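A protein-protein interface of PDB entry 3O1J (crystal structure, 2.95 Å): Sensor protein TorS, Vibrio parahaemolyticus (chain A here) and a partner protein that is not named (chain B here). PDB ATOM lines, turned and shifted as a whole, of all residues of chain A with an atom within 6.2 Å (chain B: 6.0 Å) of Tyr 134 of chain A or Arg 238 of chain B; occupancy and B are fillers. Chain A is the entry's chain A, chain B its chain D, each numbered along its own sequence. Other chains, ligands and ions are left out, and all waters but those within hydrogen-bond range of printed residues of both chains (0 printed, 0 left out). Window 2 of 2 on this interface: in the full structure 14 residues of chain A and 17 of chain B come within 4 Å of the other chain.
CG2 of Thr 131 of chain A touches CE2 of Tyr 233 of chain B (3.5 Å). CB of Arg 234 of chain B touches OG1 of Thr 131 of chain A (3.1 Å). Leu 237 of chain B touches Thr 131 of chain A. Tyr 134 of chain A touches Arg 238 of chain B (CE2 to CD, 3.5 Å).
Printed residues of chain B within 4 Å of Thr 131 of chain A: Tyr 233 (3.5 Å), Arg 234 (3.1 Å) and Leu 237 (3.98 Å). Tyr 134 of chain A touches just these residues of chain B: Arg 234 and Arg 238. Printed residues of chain A within 4 Å of Tyr 233 of chain B: Thr 131 (3.5 Å). Printed residues of chain A within 4 Å of Arg 234 of chain B: Thr 131 and Tyr 134. Gly 235 of chain B touches none of the printed residues of chain A. Printed residues of chain A within 4 Å of Leu 237 of chain B: Thr 131. Of chain A, only Tyr 134 comes within 4 Å of Arg 238 of chain B. The nearest residue of chain B that does not touch Tyr 134 of chain A is Leu 237 of chain B (4.1 Å). The nearest printed residue of chain A that does not touch Arg 238 of chain B is Glu 138 of chain A (6.9 Å).
NE of Arg 234 of chain B sits at hydrogen-bond distance from OH of Tyr 134 of chain A, 3.3 Å away.
Of the 11 printed residues of chain A, 2 touch a printed residue of chain B. Hydrophobic or aromatic side chains of chain A that line the printed part of chain B: Tyr 134. Of the 10 printed residues of chain B, 4 touch a printed residue of chain A. Hydrophobic or aromatic side chains of chain B that line the printed part of chain A: Tyr 233 and Leu 237. Along chain B the printed residues that touch a printed residue of chain A span positions 233 to 238. Among the printed residues, 5 pairs touch across the chains. Among the printed residues, no Asp or Glu carboxylate lies within 4 Å of a Lys or Arg side-chain nitrogen of the other chain.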
ATOM      1  N   ASN A 129      10.353 -21.129 -17.739  1.00  0.00           N
ATOM      2  CA  ASN A 129      10.120 -21.986 -18.903  1.00  0.00           C
ATOM      3  C   ASN A 129       9.747 -21.225 -20.170  1.00  0.00           C
ATOM      4  O   ASN A 129      10.086 -21.653 -21.279  1.00  0.00           O
ATOM      5  CB  ASN A 129       9.032 -23.022 -18.614  1.00  0.00           C
ATOM      6  CG  ASN A 129       9.449 -24.027 -17.571  1.00  0.00           C
ATOM      7  OD1 ASN A 129      10.618 -24.385 -17.475  1.00  0.00           O
ATOM      8  ND2 ASN A 129       8.491 -24.508 -16.793  1.00  0.00           N
ATOM      9  N   VAL A 130       9.036 -20.115 -20.022  1.00  0.00           N
ATOM     10  CA  VAL A 130       8.660 -19.347 -21.195  1.00  0.00           C
ATOM     11  C   VAL A 130       9.843 -18.509 -21.653  1.00  0.00           C
ATOM     12  O   VAL A 130      10.025 -18.293 -22.848  1.00  0.00           O
ATOM     13  CB  VAL A 130       7.444 -18.443 -20.924  1.00  0.00           C
ATOM     14  CG1 VAL A 130       7.263 -17.466 -22.060  1.00  0.00           C
ATOM     15  CG2 VAL A 130       6.190 -19.294 -20.790  1.00  0.00           C
ATOM     16  N   THR A 131      10.661 -18.050 -20.710  1.00  0.00           N
ATOM     17  CA  THR A 131      11.830 -17.249 -21.069  1.00  0.00           C
ATOM     18  C   THR A 131      12.716 -18.090 -21.988  1.00  0.00           C
ATOM     19  O   THR A 131      13.299 -17.594 -22.956  1.00  0.00           O
ATOM     20  CB  THR A 131      12.648 -16.846 -19.820  1.00  0.00           C
ATOM     21  OG1 THR A 131      11.837 -16.062 -18.941  1.00  0.00           O
ATOM     22  CG2 THR A 131      13.863 -16.035 -20.219  1.00  0.00           C
ATOM     23  N   HIS A 132      12.794 -19.375 -21.674  1.00  0.00           N
ATOM     24  CA  HIS A 132      13.601 -20.298 -22.439  1.00  0.00           C
ATOM     25  C   HIS A 132      13.094 -20.515 -23.854  1.00  0.00           C
ATOM     26  O   HIS A 132      13.891 -20.726 -24.770  1.00  0.00           O
ATOM     27  CB  HIS A 132      13.668 -21.630 -21.725  1.00  0.00           C
ATOM     28  CG  HIS A 132      14.483 -22.654 -22.446  1.00  0.00           C
ATOM     29  ND1 HIS A 132      13.921 -23.738 -23.087  1.00  0.00           N
ATOM     30  CD2 HIS A 132      15.822 -22.774 -22.605  1.00  0.00           C
ATOM     31  CE1 HIS A 132      14.877 -24.486 -23.605  1.00  0.00           C
ATOM     32  NE2 HIS A 132      16.040 -23.924 -23.325  1.00  0.00           N
ATOM     33  N   ILE A 133      11.777 -20.477 -24.039  1.00  0.00           N
ATOM     34  CA  ILE A 133      11.207 -20.676 -25.365  1.00  0.00           C
ATOM     35  C   ILE A 133      11.681 -19.580 -26.303  1.00  0.00           C
ATOM     36  O   ILE A 133      11.831 -19.806 -27.495  1.00  0.00           O
ATOM     37  CB  ILE A 133       9.665 -20.696 -25.328  1.00  0.00           C
ATOM     38  CG1 ILE A 133       9.189 -21.935 -24.574  1.00  0.00           C
ATOM     39  CG2 ILE A 133       9.100 -20.715 -26.740  1.00  0.00           C
ATOM     40  CD1 ILE A 133       7.696 -22.056 -24.498  1.00  0.00           C
ATOM     41  N   TYR A 134      11.930 -18.393 -25.766  1.00  0.00           N
ATOM     42  CA  TYR A 134      12.412 -17.298 -26.596  1.00  0.00           C
ATOM     43  C   TYR A 134      13.736 -17.705 -27.252  1.00  0.00           C
ATOM     44  O   TYR A 134      13.896 -17.582 -28.467  1.00  0.00           O
ATOM     45  CB  TYR A 134      12.633 -16.046 -25.756  1.00  0.00           C
ATOM     46  CG  TYR A 134      11.386 -15.393 -25.215  1.00  0.00           C
ATOM     47  CD1 TYR A 134      11.193 -15.257 -23.844  1.00  0.00           C
ATOM     48  CD2 TYR A 134      10.432 -14.843 -26.070  1.00  0.00           C
ATOM     49  CE1 TYR A 134      10.087 -14.582 -23.338  1.00  0.00           C
ATOM     50  CE2 TYR A 134       9.318 -14.164 -25.572  1.00  0.00           C
ATOM     51  CZ  TYR A 134       9.159 -14.037 -24.208  1.00  0.00           C
ATOM     52  OH  TYR A 134       8.090 -13.341 -23.701  1.00  0.00           O
ATOM     53  N   ASP A 135      14.684 -18.193 -26.450  1.00  0.00           N
ATOM     54  CA  ASP A 135      15.997 -18.607 -26.959  1.00  0.00           C
ATOM     55  C   ASP A 135      15.874 -19.626 -28.072  1.00  0.00           C
ATOM     56  O   ASP A 135      16.594 -19.553 -29.066  1.00  0.00           O
ATOM     57  CB  ASP A 135      16.858 -19.194 -25.838  1.00  0.00           C
ATOM     58  CG  ASP A 135      17.316 -18.138 -24.837  1.00  0.00           C
ATOM     59  OD1 ASP A 135      17.985 -18.514 -23.842  1.00  0.00           O
ATOM     60  OD2 ASP A 135      17.007 -16.936 -25.047  1.00  0.00           O
ATOM     61  N   LEU A 136      14.963 -20.577 -27.891  1.00  0.00           N
ATOM     62  CA  LEU A 136      14.713 -21.616 -28.883  1.00  0.00           C
ATOM     63  C   LEU A 136      14.087 -21.016 -30.130  1.00  0.00           C
ATOM     64  O   LEU A 136      14.598 -21.175 -31.232  1.00  0.00           O
ATOM     65  CB  LEU A 136      13.769 -22.680 -28.318  1.00  0.00           C
ATOM     66  CG  LEU A 136      14.328 -23.565 -27.212  1.00  0.00           C
ATOM     67  CD1 LEU A 136      13.316 -24.613 -26.826  1.00  0.00           C
ATOM     68  CD2 LEU A 136      15.594 -24.221 -27.708  1.00  0.00           C
ATOM     69  N   LEU A 137      12.972 -20.324 -29.939  1.00  0.00           N
ATOM     70  CA  LEU A 137      12.242 -19.703 -31.036  1.00  0.00           C
ATOM     71  C   LEU A 137      13.141 -18.841 -31.906  1.00  0.00           C
ATOM     72  O   LEU A 137      13.019 -18.849 -33.132  1.00  0.00           O
ATOM     73  CB  LEU A 137      11.079 -18.869 -30.481  1.00  0.00           C
ATOM     74  CG  LEU A 137      10.051 -18.239 -31.425  1.00  0.00           C
ATOM     75  CD1 LEU A 137      10.517 -16.884 -31.874  1.00  0.00           C
ATOM     76  CD2 LEU A 137       9.807 -19.153 -32.599  1.00  0.00           C
ATOM     77  N   GLU A 138      14.055 -18.105 -31.285  1.00  0.00           N
ATOM     78  CA  GLU A 138      14.939 -17.251 -32.058  1.00  0.00           C
ATOM     79  C   GLU A 138      16.327 -17.860 -32.217  1.00  0.00           C
ATOM     80  O   GLU A 138      17.350 -17.223 -31.963  1.00  0.00           O
ATOM     81  CB  GLU A 138      15.018 -15.862 -31.424  1.00  0.00           C
ATOM     82  CG  GLU A 138      15.356 -14.778 -32.436  1.00  0.00           C
ATOM     83  CD  GLU A 138      16.508 -13.913 -31.978  1.00  0.00           C
ATOM     84  OE1 GLU A 138      17.560 -14.430 -31.573  1.00  0.00           O
ATOM     85  OE2 GLU A 138      16.326 -12.590 -32.040  1.00  0.00           O
ATOM     86  N   ALA A 139      16.323 -19.118 -32.636  1.00  0.00           N
ATOM     87  CA  ALA A 139      17.512 -19.924 -32.893  1.00  0.00           C
ATOM     88  C   ALA A 139      16.943 -20.964 -33.846  1.00  0.00           C
ATOM     89  O   ALA A 139      17.550 -21.996 -34.130  1.00  0.00           O
ATOM     90  CB  ALA A 139      18.012 -20.586 -31.619  1.00  0.00           C
ATOM     91  N   TYR B 233      14.314 -10.458 -15.435  1.00  0.00           N
ATOM     92  CA  TYR B 233      15.263 -10.826 -16.466  1.00  0.00           C
ATOM     93  C   TYR B 233      14.521 -11.013 -17.781  1.00  0.00           C
ATOM     94  O   TYR B 233      14.936 -10.512 -18.822  1.00  0.00           O
ATOM     95  CB  TYR B 233      15.969 -12.132 -16.105  1.00  0.00           C
ATOM     96  CG  TYR B 233      16.659 -12.772 -17.297  1.00  0.00           C
ATOM     97  CD1 TYR B 233      17.763 -12.167 -17.902  1.00  0.00           C
ATOM     98  CD2 TYR B 233      16.173 -13.952 -17.849  1.00  0.00           C
ATOM     99  CE1 TYR B 233      18.356 -12.723 -19.026  1.00  0.00           C
ATOM    100  CE2 TYR B 233      16.755 -14.514 -18.969  1.00  0.00           C
ATOM    101  CZ  TYR B 233      17.841 -13.898 -19.552  1.00  0.00           C
ATOM    102  OH  TYR B 233      18.404 -14.466 -20.665  1.00  0.00           O
ATOM    103  N   ARG B 234      13.424 -11.755 -17.739  1.00  0.00           N
ATOM    104  CA  ARG B 234      12.649 -11.992 -18.948  1.00  0.00           C
ATOM    105  C   ARG B 234      12.142 -10.646 -19.434  1.00  0.00           C
ATOM    106  O   ARG B 234      11.861 -10.474 -20.620  1.00  0.00           O
ATOM    107  CB  ARG B 234      11.513 -12.997 -18.654  1.00  0.00           C
ATOM    108  CG  ARG B 234      10.069 -12.557 -18.906  1.00  0.00           C
ATOM    109  CD  ARG B 234       9.678 -12.718 -20.363  1.00  0.00           C
ATOM    110  NE  ARG B 234       8.343 -12.199 -20.667  1.00  0.00           N
ATOM    111  CZ  ARG B 234       7.804 -11.106 -20.130  1.00  0.00           C
ATOM    112  NH1 ARG B 234       8.452 -10.387 -19.232  1.00  0.00           N
ATOM    113  NH2 ARG B 234       6.618 -10.700 -20.526  1.00  0.00           N
ATOM    114  N   GLY B 235      12.070  -9.687 -18.509  1.00  0.00           N
ATOM    115  CA  GLY B 235      11.619  -8.343 -18.835  1.00  0.00           C
ATOM    116  C   GLY B 235      12.702  -7.599 -19.589  1.00  0.00           C
ATOM    117  O   GLY B 235      12.431  -6.934 -20.593  1.00  0.00           O
ATOM    118  N   LEU B 236      13.938  -7.702 -19.101  1.00  0.00           N
ATOM    119  CA  LEU B 236      15.079  -7.064 -19.754  1.00  0.00           C
ATOM    120  C   LEU B 236      15.218  -7.686 -21.133  1.00  0.00           C
ATOM    121  O   LEU B 236      15.317  -6.994 -22.142  1.00  0.00           O
ATOM    122  CB  LEU B 236      16.362  -7.320 -18.965  1.00  0.00           C
ATOM    123  CG  LEU B 236      16.483  -6.584 -17.635  1.00  0.00           C
ATOM    124  CD1 LEU B 236      17.633  -7.168 -16.830  1.00  0.00           C
ATOM    125  CD2 LEU B 236      16.671  -5.090 -17.900  1.00  0.00           C
ATOM    126  N   LEU B 237      15.215  -9.011 -21.157  1.00  0.00           N
ATOM    127  CA  LEU B 237      15.334  -9.751 -22.392  1.00  0.00           C
ATOM    128  C   LEU B 237      14.370  -9.269 -23.468  1.00  0.00           C
ATOM    129  O   LEU B 237      14.714  -9.224 -24.637  1.00  0.00           O
ATOM    130  CB  LEU B 237      15.072 -11.230 -22.133  1.00  0.00           C
ATOM    131  CG  LEU B 237      15.265 -12.079 -23.386  1.00  0.00           C
ATOM    132  CD1 LEU B 237      16.734 -12.018 -23.789  1.00  0.00           C
ATOM    133  CD2 LEU B 237      14.830 -13.502 -23.128  1.00  0.00           C
ATOM    134  N   ARG B 238      13.160  -8.901 -23.072  1.00  0.00           N
ATOM    135  CA  ARG B 238      12.150  -8.474 -24.032  1.00  0.00           C
ATOM    136  C   ARG B 238      11.874  -6.978 -24.023  1.00  0.00           C
ATOM    137  O   ARG B 238      10.786  -6.548 -24.389  1.00  0.00           O
ATOM    138  CB  ARG B 238      10.853  -9.230 -23.756  1.00  0.00           C
ATOM    139  CG  ARG B 238      10.970 -10.754 -23.832  1.00  0.00           C
ATOM    140  CD  ARG B 238      11.054 -11.183 -25.263  1.00  0.00           C
ATOM    141  NE  ARG B 238      10.013 -10.505 -26.018  1.00  0.00           N
ATOM    142  CZ  ARG B 238      10.109 -10.186 -27.303  1.00  0.00           C
ATOM    143  NH1 ARG B 238      11.206 -10.490 -27.983  1.00  0.00           N
ATOM    144  NH2 ARG B 238       9.120  -9.535 -27.900  1.00  0.00           N
ATOM    145  N   ASN B 239      12.855  -6.191 -23.595  1.00  0.00           N
ATOM    146  CA  ASN B 239      12.737  -4.735 -23.545  1.00  0.00           C
ATOM    147  C   ASN B 239      11.508  -4.182 -22.870  1.00  0.00           C
ATOM    148  O   ASN B 239      10.845  -3.308 -23.418  1.00  0.00           O
ATOM    149  CB  ASN B 239      12.815  -4.147 -24.945  1.00  0.00           C
ATOM    150  CG  ASN B 239      14.198  -4.247 -25.530  1.00  0.00           C
ATOM    151  OD1 ASN B 239      14.622  -5.314 -25.980  1.00  0.00           O
ATOM    152  ND2 ASN B 239      14.925  -3.132 -25.513  1.00  0.00           N
ATOM    153  N   LYS B 240      11.211  -4.685 -21.679  1.00  0.00           N
ATOM    154  CA  LYS B 240      10.070  -4.218 -20.908  1.00  0.00           C
ATOM    155  C   LYS B 240      10.586  -3.615 -19.602  1.00  0.00           C
ATOM    156  O   LYS B 240       9.888  -2.875 -18.913  1.00  0.00           O
ATOM    157  CB  LYS B 240       9.130  -5.378 -20.634  1.00  0.00           C
ATOM    158  CG  LYS B 240       8.490  -5.959 -21.888  1.00  0.00           C
ATOM    159  CD  LYS B 240       7.528  -4.967 -22.533  1.00  0.00           C
ATOM    160  CE  LYS B 240       6.544  -5.665 -23.471  1.00  0.00           C
ATOM    161  NZ  LYS B 240       7.254  -6.511 -24.474  1.00  0.00           N
ATOM    162  N   VAL B 241      11.831  -3.943 -19.280  1.00  0.00           N
ATOM    163  CA  VAL B 241      12.515  -3.436 -18.098  1.00  0.00           C
ATOM    164  C   VAL B 241      13.775  -2.727 -18.606  1.00  0.00           C
ATOM    165  O   VAL B 241      14.456  -3.241 -19.499  1.00  0.00           O
ATOM    166  CB  VAL B 241      12.915  -4.584 -17.173  1.00  0.00           C
ATOM    167  CG1 VAL B 241      13.855  -4.089 -16.095  1.00  0.00           C
ATOM    168  CG2 VAL B 241      11.676  -5.177 -16.550  1.00  0.00           C
ATOM    169  N   PRO B 282      18.809  -4.328 -21.282  1.00  0.00           N
ATOM    170  CA  PRO B 282      18.415  -5.243 -22.352  1.00  0.00           C
ATOM    171  C   PRO B 282      19.516  -5.592 -23.361  1.00  0.00           C
ATOM    172  O   PRO B 282      19.560  -6.713 -23.866  1.00  0.00           O
ATOM    173  CB  PRO B 282      17.211  -4.538 -22.986  1.00  0.00           C
ATOM    174  CG  PRO B 282      17.433  -3.092 -22.638  1.00  0.00           C
ATOM    175  CD  PRO B 282      17.916  -3.162 -21.224  1.00  0.00           C
